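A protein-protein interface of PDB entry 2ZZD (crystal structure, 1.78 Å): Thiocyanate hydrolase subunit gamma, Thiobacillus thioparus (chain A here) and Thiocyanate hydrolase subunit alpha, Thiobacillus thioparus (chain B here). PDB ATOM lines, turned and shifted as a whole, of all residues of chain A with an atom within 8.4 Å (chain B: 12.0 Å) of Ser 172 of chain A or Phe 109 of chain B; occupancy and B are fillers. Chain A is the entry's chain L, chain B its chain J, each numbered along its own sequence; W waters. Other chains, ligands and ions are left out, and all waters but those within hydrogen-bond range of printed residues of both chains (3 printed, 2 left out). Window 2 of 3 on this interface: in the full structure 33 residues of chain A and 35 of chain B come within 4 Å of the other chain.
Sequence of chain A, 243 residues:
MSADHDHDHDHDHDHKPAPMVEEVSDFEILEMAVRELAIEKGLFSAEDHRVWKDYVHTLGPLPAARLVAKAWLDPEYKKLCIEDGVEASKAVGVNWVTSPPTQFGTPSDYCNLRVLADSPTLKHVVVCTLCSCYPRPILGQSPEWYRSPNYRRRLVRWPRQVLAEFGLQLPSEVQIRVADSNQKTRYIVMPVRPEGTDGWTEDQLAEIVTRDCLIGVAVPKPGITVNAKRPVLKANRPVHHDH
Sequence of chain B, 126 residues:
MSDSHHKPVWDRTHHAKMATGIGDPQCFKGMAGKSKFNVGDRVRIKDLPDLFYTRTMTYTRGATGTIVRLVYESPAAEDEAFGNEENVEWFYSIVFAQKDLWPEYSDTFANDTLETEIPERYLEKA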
ATOM      1  N   THR A 121      16.811  10.584  -9.083  1.00  0.00           N
ATOM      2  CA  THR A 121      18.188  10.921  -8.720  1.00  0.00           C
ATOM      3  C   THR A 121      18.442  12.413  -8.513  1.00  0.00           C
ATOM      4  O   THR A 121      19.588  12.824  -8.327  1.00  0.00           O
ATOM      5  CB  THR A 121      19.180  10.458  -9.804  1.00  0.00           C
ATOM      6  OG1 THR A 121      18.865  11.104 -11.046  1.00  0.00           O
ATOM      7  CG2 THR A 121      19.114   8.956  -9.979  1.00  0.00           C
ATOM      8  N   PRO A 159      21.664  22.472   2.987  1.00  0.00           N
ATOM      9  CA  PRO A 159      20.322  22.110   2.521  1.00  0.00           C
ATOM     10  C   PRO A 159      19.710  20.866   3.143  1.00  0.00           C
ATOM     11  O   PRO A 159      18.519  20.849   3.446  1.00  0.00           O
ATOM     12  CB  PRO A 159      20.499  21.980   1.011  1.00  0.00           C
ATOM     13  CG  PRO A 159      21.926  21.524   0.877  1.00  0.00           C
ATOM     14  CD  PRO A 159      22.636  22.410   1.881  1.00  0.00           C
ATOM     15  N   ARG A 160      20.499  19.819   3.337  1.00  0.00           N
ATOM     16  CA  ARG A 160      19.925  18.616   3.917  1.00  0.00           C
ATOM     17  C   ARG A 160      19.502  18.816   5.355  1.00  0.00           C
ATOM     18  O   ARG A 160      18.523  18.218   5.806  1.00  0.00           O
ATOM     19  CB  ARG A 160      20.895  17.452   3.799  1.00  0.00           C
ATOM     20  CG  ARG A 160      20.915  16.914   2.390  1.00  0.00           C
ATOM     21  CD  ARG A 160      21.805  15.722   2.264  1.00  0.00           C
ATOM     22  NE  ARG A 160      21.977  15.349   0.867  1.00  0.00           N
ATOM     23  CZ  ARG A 160      21.322  14.363   0.267  1.00  0.00           C
ATOM     24  NH1 ARG A 160      20.436  13.634   0.939  1.00  0.00           N
ATOM     25  NH2 ARG A 160      21.566  14.095  -1.008  1.00  0.00           N
ATOM     26  N   GLN A 161      20.227  19.663   6.074  1.00  0.00           N
ATOM     27  CA  GLN A 161      19.880  19.932   7.457  1.00  0.00           C
ATOM     28  C   GLN A 161      18.612  20.790   7.512  1.00  0.00           C
ATOM     29  O   GLN A 161      17.702  20.505   8.287  1.00  0.00           O
ATOM     30  CB  GLN A 161      21.050  20.616   8.177  1.00  0.00           C
ATOM     31  CG  GLN A 161      22.269  19.709   8.370  1.00  0.00           C
ATOM     32  CD  GLN A 161      23.171  19.622   7.146  1.00  0.00           C
ATOM     33  OE1 GLN A 161      22.880  20.193   6.094  1.00  0.00           O
ATOM     34  NE2 GLN A 161      24.280  18.902   7.283  1.00  0.00           N
ATOM     35  N   GLN A 169      13.634  14.337   3.887  1.00  0.00           N
ATOM     36  CA  GLN A 169      14.929  13.689   3.800  1.00  0.00           C
ATOM     37  C   GLN A 169      14.971  12.872   2.524  1.00  0.00           C
ATOM     38  O   GLN A 169      13.984  12.251   2.128  1.00  0.00           O
ATOM     39  CB  GLN A 169      15.155  12.774   5.014  1.00  0.00           C
ATOM     40  CG  GLN A 169      16.600  12.313   5.226  1.00  0.00           C
ATOM     41  CD  GLN A 169      16.795  11.576   6.553  1.00  0.00           C
ATOM     42  OE1 GLN A 169      17.379  12.111   7.501  1.00  0.00           O
ATOM     43  NE2 GLN A 169      16.296  10.349   6.622  1.00  0.00           N
ATOM     44  N   LEU A 170      16.116  12.885   1.868  1.00  0.00           N
ATOM     45  CA  LEU A 170      16.270  12.125   0.647  1.00  0.00           C
ATOM     46  C   LEU A 170      17.486  11.232   0.757  1.00  0.00           C
ATOM     47  O   LEU A 170      18.395  11.531   1.518  1.00  0.00           O
ATOM     48  CB  LEU A 170      16.394  13.082  -0.536  1.00  0.00           C
ATOM     49  CG  LEU A 170      14.990  13.563  -0.788  1.00  0.00           C
ATOM     50  CD1 LEU A 170      14.870  15.067  -0.688  1.00  0.00           C
ATOM     51  CD2 LEU A 170      14.511  13.013  -2.109  1.00  0.00           C
ATOM     52  N   PRO A 171      17.522  10.130  -0.016  1.00  0.00           N
ATOM     53  CA  PRO A 171      18.679   9.232   0.052  1.00  0.00           C
ATOM     54  C   PRO A 171      19.972  10.034  -0.136  1.00  0.00           C
ATOM     55  O   PRO A 171      19.998  11.034  -0.862  1.00  0.00           O
ATOM     56  CB  PRO A 171      18.431   8.266  -1.100  1.00  0.00           C
ATOM     57  CG  PRO A 171      16.923   8.186  -1.139  1.00  0.00           C
ATOM     58  CD  PRO A 171      16.539   9.648  -1.006  1.00  0.00           C
ATOM     59  N   SER A 172      21.049   9.586   0.497  1.00  0.00           N
ATOM     60  CA  SER A 172      22.317  10.292   0.399  1.00  0.00           C
ATOM     61  C   SER A 172      22.889  10.364  -1.011  1.00  0.00           C
ATOM     62  O   SER A 172      23.593  11.314  -1.336  1.00  0.00           O
ATOM     63  CB  SER A 172      23.348   9.666   1.343  1.00  0.00           C
ATOM     64  OG  SER A 172      23.638   8.330   0.968  1.00  0.00           O
ATOM     65  N   GLU A 173      22.589   9.371  -1.846  1.00  0.00           N
ATOM     66  CA  GLU A 173      23.105   9.363  -3.211  1.00  0.00           C
ATOM     67  C   GLU A 173      22.305  10.245  -4.163  1.00  0.00           C
ATOM     68  O   GLU A 173      22.772  10.574  -5.253  1.00  0.00           O
ATOM     69  CB  GLU A 173      23.163   7.933  -3.753  1.00  0.00           C
ATOM     70  CG  GLU A 173      24.299   7.112  -3.157  1.00  0.00           C
ATOM     71  CD  GLU A 173      25.667   7.684  -3.488  1.00  0.00           C
ATOM     72  OE1 GLU A 173      26.567   7.627  -2.623  1.00  0.00           O
ATOM     73  OE2 GLU A 173      25.844   8.182  -4.621  1.00  0.00           O
ATOM     74  N   VAL A 174      21.097  10.617  -3.754  1.00  0.00           N
ATOM     75  CA  VAL A 174      20.265  11.482  -4.576  1.00  0.00           C
ATOM     76  C   VAL A 174      20.898  12.868  -4.575  1.00  0.00           C
ATOM     77  O   VAL A 174      21.381  13.335  -3.544  1.00  0.00           O
ATOM     78  CB  VAL A 174      18.829  11.591  -4.015  1.00  0.00           C
ATOM     79  CG1 VAL A 174      18.101  12.763  -4.654  1.00  0.00           C
ATOM     80  CG2 VAL A 174      18.070  10.311  -4.297  1.00  0.00           C
ATOM     81  N   GLN A 175      20.903  13.516  -5.733  1.00  0.00           N
ATOM     82  CA  GLN A 175      21.466  14.847  -5.846  1.00  0.00           C
ATOM     83  C   GLN A 175      20.473  15.905  -5.393  1.00  0.00           C
ATOM     84  O   GLN A 175      19.428  16.087  -6.014  1.00  0.00           O
ATOM     85  CB  GLN A 175      21.873  15.139  -7.299  1.00  0.00           C
ATOM     86  CG  GLN A 175      22.194  16.615  -7.573  1.00  0.00           C
ATOM     87  CD  GLN A 175      22.531  16.890  -9.032  1.00  0.00           C
ATOM     88  OE1 GLN A 175      22.516  15.985  -9.875  1.00  0.00           O
ATOM     89  NE2 GLN A 175      22.831  18.144  -9.340  1.00  0.00           N
ATOM     90  N   ILE A 176      20.772  16.579  -4.288  1.00  0.00           N
ATOM     91  CA  ILE A 176      19.901  17.660  -3.859  1.00  0.00           C
ATOM     92  C   ILE A 176      20.494  18.875  -4.556  1.00  0.00           C
ATOM     93  O   ILE A 176      21.695  19.132  -4.437  1.00  0.00           O
ATOM     94  CB  ILE A 176      19.965  17.918  -2.334  1.00  0.00           C
ATOM     95  CG1 ILE A 176      19.312  16.770  -1.559  1.00  0.00           C
ATOM     96  CG2 ILE A 176      19.257  19.236  -2.007  1.00  0.00           C
ATOM     97  CD1 ILE A 176      17.803  16.694  -1.699  1.00  0.00           C
ATOM     98  N   VAL B  95      26.194  25.315 -12.612  1.00  0.00           N
ATOM     99  CA  VAL B  95      26.031  24.319 -11.560  1.00  0.00           C
ATOM    100  C   VAL B  95      27.369  24.057 -10.866  1.00  0.00           C
ATOM    101  O   VAL B  95      28.366  23.731 -11.515  1.00  0.00           O
ATOM    102  CB  VAL B  95      25.479  22.985 -12.123  1.00  0.00           C
ATOM    103  CG1 VAL B  95      25.512  21.905 -11.047  1.00  0.00           C
ATOM    104  CG2 VAL B  95      24.045  23.183 -12.609  1.00  0.00           C
ATOM    105  N   PHE B  96      27.372  24.217  -9.545  1.00  0.00           N
ATOM    106  CA  PHE B  96      28.555  24.006  -8.712  1.00  0.00           C
ATOM    107  C   PHE B  96      28.376  22.767  -7.843  1.00  0.00           C
ATOM    108  O   PHE B  96      27.271  22.480  -7.382  1.00  0.00           O
ATOM    109  CB  PHE B  96      28.753  25.180  -7.754  1.00  0.00           C
ATOM    110  CG  PHE B  96      28.994  26.494  -8.424  1.00  0.00           C
ATOM    111  CD1 PHE B  96      30.279  26.876  -8.796  1.00  0.00           C
ATOM    112  CD2 PHE B  96      27.941  27.378  -8.631  1.00  0.00           C
ATOM    113  CE1 PHE B  96      30.514  28.128  -9.361  1.00  0.00           C
ATOM    114  CE2 PHE B  96      28.161  28.631  -9.196  1.00  0.00           C
ATOM    115  CZ  PHE B  96      29.451  29.009  -9.561  1.00  0.00           C
ATOM    116  N   ALA B  97      29.462  22.040  -7.608  1.00  0.00           N
ATOM    117  CA  ALA B  97      29.396  20.887  -6.722  1.00  0.00           C
ATOM    118  C   ALA B  97      29.459  21.525  -5.330  1.00  0.00           C
ATOM    119  O   ALA B  97      30.291  22.400  -5.096  1.00  0.00           O
ATOM    120  CB  ALA B  97      30.594  19.972  -6.944  1.00  0.00           C
ATOM    121  N   GLN B  98      28.588  21.109  -4.416  1.00  0.00           N
ATOM    122  CA  GLN B  98      28.590  21.694  -3.080  1.00  0.00           C
ATOM    123  C   GLN B  98      29.955  21.621  -2.401  1.00  0.00           C
ATOM    124  O   GLN B  98      30.352  22.550  -1.702  1.00  0.00           O
ATOM    125  CB  GLN B  98      27.523  21.028  -2.205  1.00  0.00           C
ATOM    126  CG  GLN B  98      26.091  21.430  -2.572  1.00  0.00           C
ATOM    127  CD  GLN B  98      25.732  22.834  -2.098  1.00  0.00           C
ATOM    128  OE1 GLN B  98      26.511  23.774  -2.260  1.00  0.00           O
ATOM    129  NE2 GLN B  98      24.541  22.983  -1.522  1.00  0.00           N
ATOM    130  N   LYS B  99      30.676  20.525  -2.620  1.00  0.00           N
ATOM    131  CA  LYS B  99      31.995  20.342  -2.019  1.00  0.00           C
ATOM    132  C   LYS B  99      32.979  21.418  -2.475  1.00  0.00           C
ATOM    133  O   LYS B  99      33.957  21.700  -1.786  1.00  0.00           O
ATOM    134  CB  LYS B  99      32.555  18.961  -2.381  1.00  0.00           C
ATOM    135  CG  LYS B  99      32.870  18.821  -3.858  1.00  0.00           C
ATOM    136  CD  LYS B  99      32.934  17.372  -4.323  1.00  0.00           C
ATOM    137  CE  LYS B  99      34.214  16.667  -3.896  1.00  0.00           C
ATOM    138  NZ  LYS B  99      34.194  16.223  -2.477  1.00  0.00           N
ATOM    139  N   ASP B 100      32.730  22.019  -3.636  1.00  0.00           N
ATOM    140  CA  ASP B 100      33.630  23.052  -4.133  1.00  0.00           C
ATOM    141  C   ASP B 100      33.320  24.429  -3.556  1.00  0.00           C
ATOM    142  O   ASP B 100      34.088  25.372  -3.735  1.00  0.00           O
ATOM    143  CB  ASP B 100      33.602  23.111  -5.663  1.00  0.00           C
ATOM    144  CG  ASP B 100      34.235  21.887  -6.304  1.00  0.00           C
ATOM    145  OD1 ASP B 100      35.165  21.315  -5.699  1.00  0.00           O
ATOM    146  OD2 ASP B 100      33.817  21.505  -7.420  1.00  0.00           O
ATOM    147  N   LEU B 101      32.191  24.547  -2.869  1.00  0.00           N
ATOM    148  CA  LEU B 101      31.810  25.810  -2.256  1.00  0.00           C
ATOM    149  C   LEU B 101      32.080  25.779  -0.758  1.00  0.00           C
ATOM    150  O   LEU B 101      32.627  26.728  -0.189  1.00  0.00           O
ATOM    151  CB  LEU B 101      30.316  26.081  -2.477  1.00  0.00           C
ATOM    152  CG  LEU B 101      29.848  26.261  -3.923  1.00  0.00           C
ATOM    153  CD1 LEU B 101      28.343  26.535  -3.948  1.00  0.00           C
ATOM    154  CD2 LEU B 101      30.604  27.420  -4.559  1.00  0.00           C
ATOM    155  N   TRP B 102      31.704  24.672  -0.130  1.00  0.00           N
ATOM    156  CA  TRP B 102      31.827  24.534   1.314  1.00  0.00           C
ATOM    157  C   TRP B 102      32.834  23.449   1.707  1.00  0.00           C
ATOM    158  O   TRP B 102      32.600  22.259   1.483  1.00  0.00           O
ATOM    159  CB  TRP B 102      30.439  24.221   1.890  1.00  0.00           C
ATOM    160  CG  TRP B 102      29.317  24.934   1.159  1.00  0.00           C
ATOM    161  CD1 TRP B 102      28.342  24.357   0.389  1.00  0.00           C
ATOM    162  CD2 TRP B 102      29.071  26.348   1.116  1.00  0.00           C
ATOM    163  NE1 TRP B 102      27.510  25.322  -0.130  1.00  0.00           N
ATOM    164  CE2 TRP B 102      27.934  26.552   0.299  1.00  0.00           C
ATOM    165  CE3 TRP B 102      29.703  27.463   1.685  1.00  0.00           C
ATOM    166  CZ2 TRP B 102      27.412  27.827   0.041  1.00  0.00           C
ATOM    167  CZ3 TRP B 102      29.184  28.731   1.428  1.00  0.00           C
ATOM    168  CH2 TRP B 102      28.049  28.901   0.612  1.00  0.00           C
ATOM    169  N   PRO B 103      33.973  23.853   2.300  1.00  0.00           N
ATOM    170  CA  PRO B 103      35.032  22.935   2.729  1.00  0.00           C
ATOM    171  C   PRO B 103      34.549  21.753   3.557  1.00  0.00           C
ATOM    172  O   PRO B 103      35.066  20.638   3.420  1.00  0.00           O
ATOM    173  CB  PRO B 103      35.971  23.836   3.534  1.00  0.00           C
ATOM    174  CG  PRO B 103      35.831  25.159   2.846  1.00  0.00           C
ATOM    175  CD  PRO B 103      34.328  25.245   2.637  1.00  0.00           C
ATOM    176  N   GLU B 104      33.561  22.002   4.411  1.00  0.00           N
ATOM    177  CA  GLU B 104      33.028  20.972   5.297  1.00  0.00           C
ATOM    178  C   GLU B 104      31.988  20.024   4.700  1.00  0.00           C
ATOM    179  O   GLU B 104      31.595  19.059   5.354  1.00  0.00           O
ATOM    180  CB  GLU B 104      32.427  21.620   6.551  1.00  0.00           C
ATOM    181  CG  GLU B 104      31.017  22.186   6.378  1.00  0.00           C
ATOM    182  CD  GLU B 104      30.973  23.518   5.646  1.00  0.00           C
ATOM    183  OE1 GLU B 104      32.042  24.063   5.291  1.00  0.00           O
ATOM    184  OE2 GLU B 104      29.852  24.031   5.439  1.00  0.00           O
ATOM    185  N   TYR B 105      31.543  20.279   3.472  1.00  0.00           N
ATOM    186  CA  TYR B 105      30.528  19.411   2.879  1.00  0.00           C
ATOM    187  C   TYR B 105      30.951  17.943   2.928  1.00  0.00           C
ATOM    188  O   TYR B 105      32.076  17.595   2.572  1.00  0.00           O
ATOM    189  CB  TYR B 105      30.218  19.823   1.439  1.00  0.00           C
ATOM    190  CG  TYR B 105      28.744  19.690   1.131  1.00  0.00           C
ATOM    191  CD1 TYR B 105      27.833  20.643   1.587  1.00  0.00           C
ATOM    192  CD2 TYR B 105      28.249  18.576   0.451  1.00  0.00           C
ATOM    193  CE1 TYR B 105      26.463  20.492   1.379  1.00  0.00           C
ATOM    194  CE2 TYR B 105      26.881  18.412   0.241  1.00  0.00           C
ATOM    195  CZ  TYR B 105      25.993  19.374   0.709  1.00  0.00           C
ATOM    196  OH  TYR B 105      24.637  19.209   0.523  1.00  0.00           O
ATOM    197  N   SER B 106      30.034  17.086   3.368  1.00  0.00           N
ATOM    198  CA  SER B 106      30.309  15.659   3.508  1.00  0.00           C
ATOM    199  C   SER B 106      30.353  14.837   2.223  1.00  0.00           C
ATOM    200  O   SER B 106      29.508  14.992   1.337  1.00  0.00           O
ATOM    201  CB  SER B 106      29.293  15.024   4.457  1.00  0.00           C
ATOM    202  OG  SER B 106      29.509  13.623   4.553  1.00  0.00           O
ATOM    203  N   ASP B 107      31.346  13.952   2.140  1.00  0.00           N
ATOM    204  CA  ASP B 107      31.504  13.075   0.986  1.00  0.00           C
ATOM    205  C   ASP B 107      30.296  12.152   0.877  1.00  0.00           C
ATOM    206  O   ASP B 107      30.055  11.561  -0.174  1.00  0.00           O
ATOM    207  CB  ASP B 107      32.764  12.210   1.105  1.00  0.00           C
ATOM    208  CG  ASP B 107      34.047  13.004   0.944  1.00  0.00           C
ATOM    209  OD1 ASP B 107      34.007  14.120   0.388  1.00  0.00           O
ATOM    210  OD2 ASP B 107      35.109  12.489   1.359  1.00  0.00           O
ATOM    211  N   THR B 108      29.553  12.013   1.972  1.00  0.00           N
ATOM    212  CA  THR B 108      28.372  11.157   1.976  1.00  0.00           C
ATOM    213  C   THR B 108      27.329  11.695   1.002  1.00  0.00           C
ATOM    214  O   THR B 108      26.598  10.930   0.377  1.00  0.00           O
ATOM    215  CB  THR B 108      27.755  11.053   3.388  1.00  0.00           C
ATOM    216  OG1 THR B 108      28.657  10.350   4.252  1.00  0.00           O
ATOM    217  CG2 THR B 108      26.430  10.302   3.343  1.00  0.00           C
ATOM    218  N   PHE B 109      27.275  13.014   0.873  1.00  0.00           N
ATOM    219  CA  PHE B 109      26.334  13.667  -0.033  1.00  0.00           C
ATOM    220  C   PHE B 109      27.132  14.169  -1.236  1.00  0.00           C
ATOM    221  O   PHE B 109      27.085  15.340  -1.606  1.00  0.00           O
ATOM    222  CB  PHE B 109      25.648  14.811   0.713  1.00  0.00           C
ATOM    223  CG  PHE B 109      25.027  14.378   2.014  1.00  0.00           C
ATOM    224  CD1 PHE B 109      24.038  13.393   2.030  1.00  0.00           C
ATOM    225  CD2 PHE B 109      25.452  14.919   3.224  1.00  0.00           C
ATOM    226  CE1 PHE B 109      23.484  12.953   3.234  1.00  0.00           C
ATOM    227  CE2 PHE B 109      24.903  14.486   4.432  1.00  0.00           C
ATOM    228  CZ  PHE B 109      23.916  13.499   4.435  1.00  0.00           C
ATOM    229  N   ALA B 110      27.853  13.227  -1.840  1.00  0.00           N
ATOM    230  CA  ALA B 110      28.733  13.449  -2.982  1.00  0.00           C
ATOM    231  C   ALA B 110      28.144  14.094  -4.234  1.00  0.00           C
ATOM    232  O   ALA B 110      28.874  14.735  -4.998  1.00  0.00           O
ATOM    233  CB  ALA B 110      29.393  12.121  -3.363  1.00  0.00           C
ATOM    234  N   ASN B 111      26.842  13.942  -4.454  1.00  0.00           N
ATOM    235  CA  ASN B 111      26.235  14.490  -5.666  1.00  0.00           C
ATOM    236  C   ASN B 111      25.475  15.808  -5.538  1.00  0.00           C
ATOM    237  O   ASN B 111      24.962  16.324  -6.533  1.00  0.00           O
ATOM    238  CB  ASN B 111      25.328  13.424  -6.296  1.00  0.00           C
ATOM    239  CG  ASN B 111      26.062  12.116  -6.535  1.00  0.00           C
ATOM    240  OD1 ASN B 111      27.163  12.110  -7.082  1.00  0.00           O
ATOM    241  ND2 ASN B 111      25.460  11.002  -6.124  1.00  0.00           N
ATOM    242  N   ASP B 112      25.426  16.371  -4.334  1.00  0.00           N
ATOM    243  CA  ASP B 112      24.702  17.628  -4.127  1.00  0.00           C
ATOM    244  C   ASP B 112      25.315  18.799  -4.888  1.00  0.00           C
ATOM    245  O   ASP B 112      26.536  18.909  -5.008  1.00  0.00           O
ATOM    246  CB  ASP B 112      24.624  17.953  -2.638  1.00  0.00           C
ATOM    247  CG  ASP B 112      23.736  16.981  -1.881  1.00  0.00           C
ATOM    248  OD1 ASP B 112      23.146  16.084  -2.527  1.00  0.00           O
ATOM    249  OD2 ASP B 112      23.617  17.117  -0.643  1.00  0.00           O
ATOM    250  N   THR B 113      24.455  19.684  -5.387  1.00  0.00           N
ATOM    251  CA  THR B 113      24.895  20.833  -6.170  1.00  0.00           C
ATOM    252  C   THR B 113      24.127  22.116  -5.870  1.00  0.00           C
ATOM    253  O   THR B 113      23.129  22.115  -5.144  1.00  0.00           O
ATOM    254  CB  THR B 113      24.719  20.564  -7.675  1.00  0.00           C
ATOM    255  OG1 THR B 113      23.346  20.234  -7.936  1.00  0.00           O
ATOM    256  CG2 THR B 113      25.608  19.418  -8.123  1.00  0.00           C
ATOM    257  N   LEU B 114      24.612  23.209  -6.448  1.00  0.00           N
ATOM    258  CA  LEU B 114      23.979  24.513  -6.316  1.00  0.00           C
ATOM    259  C   LEU B 114      23.970  25.126  -7.709  1.00  0.00           C
ATOM    260  O   LEU B 114      24.997  25.162  -8.385  1.00  0.00           O
ATOM    261  CB  LEU B 114      24.749  25.422  -5.348  1.00  0.00           C
ATOM    262  CG  LEU B 114      24.118  26.810  -5.153  1.00  0.00           C
ATOM    263  CD1 LEU B 114      24.300  27.267  -3.719  1.00  0.00           C
ATOM    264  CD2 LEU B 114      24.718  27.810  -6.132  1.00  0.00           C
HETATM  265  O   HOH W   1      23.414  19.489   3.132  1.00  0.00           O
HETATM  266  O   HOH W   2      22.686  20.959  -2.594  1.00  0.00           O
HETATM  267  O   HOH W   3      26.120   8.381  -0.139  1.00  0.00           O
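The side-chain amide nitrogen of Asn 111 of chain B lies within hydrogen-bond range of the backbone carbonyl oxygen of Glu 173 of chain A. The guanidinium group (NE) of Arg 160 of chain A is in salt-bridge range of the side-chain carboxylate (OD2) of Asp 112 of chain B (2.8 Å). OD1 of Asp 112 of chain B lies within hydrogen-bond range of N of Ile 176 of chain A (3.0 Å). The side-chain hydroxyl of Thr 113 of chain B sits at hydrogen-bond distance from the side-chain amide nitrogen of Gln 175 of chain A (2.6 Å). N of Thr 113 of chain B is in hydrogen-bond range of O of Ile 176 of chain A (3.0 Å). O of Ser 172 of chain A lies close to O of Thr 108 of chain B, at 3.5 Å. The backbone carbonyl oxygen (O) of Val 174 of chain A sits close to the side-chain carboxylate (OD1) of Asp 112 of chain B (3.4 Å).
The side-chain amide oxygen of Gln 98 of chain B lies within hydrogen-bond range of the indole nitrogen of Trp 102 of chain B, at 2.8 Å. The backbone NH (N) of Gln 98 of chain B is in hydrogen-bond range of the backbone carbonyl oxygen (O) of Asp 112 of chain B (3.1 Å). OH of Tyr 105 of chain B sits at hydrogen-bond distance from OD2 of Asp 112 of chain B (2.6 Å). The backbone NH (N) of Thr 108 of chain B sits close to the side-chain hydroxyl (OG) of Ser 106 of chain B, 3.0 Å away. The backbone carbonyl oxygen (O) of Leu 170 of chain A sits at hydrogen-bond distance from the guanidinium group (NH1) of Arg 160 of chain A. The guanidinium group (NH1) of Arg 160 of chain A sits at hydrogen-bond distance from the backbone carbonyl oxygen (O) of Pro 171 of chain A, at 3.2 Å.
Pro 159 of chain A touches Gln 98 of chain B. OH of Tyr 105 of chain B touches CG of Pro 159 of chain A, 3.6 Å away. CD1 of Phe 109 of chain B touches NE of Arg 160 of chain A, at 3.1 Å. Ser 172 of chain A touches Phe 109 of chain B (CB to CE1, 3.8 Å). Gln 175 of chain A touches Asn 111 of chain B (CG to O, 3.0 Å). Asp 112 of chain B touches Gln 175 of chain A (OD1 to CA, 3.9 Å).
Of chain B, only Thr 108 (3.5 Å) and Phe 109 (3.8 Å) come within 4 Å of Ser 172 of chain A. Of chain A, only Arg 160 (3.1 Å) and Ser 172 (3.8 Å) come within 4 Å of Phe 109 of chain B. Arg 160 of chain A touches just these residues of chain B: Phe 109 (3.1 Å) and Asp 112 (2.8 Å). No residue of chain B comes within 4 Å of Pro 171 of chain A. Of chain B, only Asp 112 (3.4 Å) comes within 4 Å of Val 174 of chain A. No residue of chain A comes within 4 Å of Ala 110 of chain B. Printed residues of chain A within 4 Å of Thr 113 of chain B: Gln 175 (2.6 Å) and Ile 176 (3.0 Å). Of the printed residues of chain B, Ile 176 of chain A touches Asp 112 (3.0 Å) and Thr 113 (3.0 Å). Of the printed residues of chain A, Asp 112 of chain B touches Arg 160, Val 174, Gln 175 and Ile 176. Lys 99 of chain B touches none of the printed residues of chain A. The nearest residue of chain B that does not touch Ser 172 of chain A is Ala 110 of chain B (4.7 Å). The nearest printed residue of chain A that does not touch Asp 112 of chain B is Ser 172 of chain A (4.9 Å).
Of the 20 printed residues of chain B, 7 touch a printed residue of chain A. Hydrophobic or aromatic side chains of chain B within 4 Å of the printed part of chain A: Tyr 105 and Phe 109. Of the 12 printed residues of chain A, 7 touch a printed residue of chain B. Hydrophobic or aromatic side chains of chain A within 4 Å of the printed part of chain B: Pro 159 and Ile 176.
Water W3 lies within hydrogen-bond range of OE1 of Glu 173 of chain A (2.6 Å), O of Thr 108 of chain B (2.6 Å) and OG of Ser 172 of chain A (2.7 Å). Water W2 lies within hydrogen-bond range of O of Ile 176 of chain A (2.8 Å), O of Thr 113 of chain B (2.8 Å) and NE2 of Gln 98 of chain B (2.9 Å). Water W1 lies within hydrogen-bond range of OH of Tyr 105 of chain B (2.9 Å), N of Arg 160 of chain A (2.9 Å) and OE1 of Gln 161 of chain A (3.1 Å).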
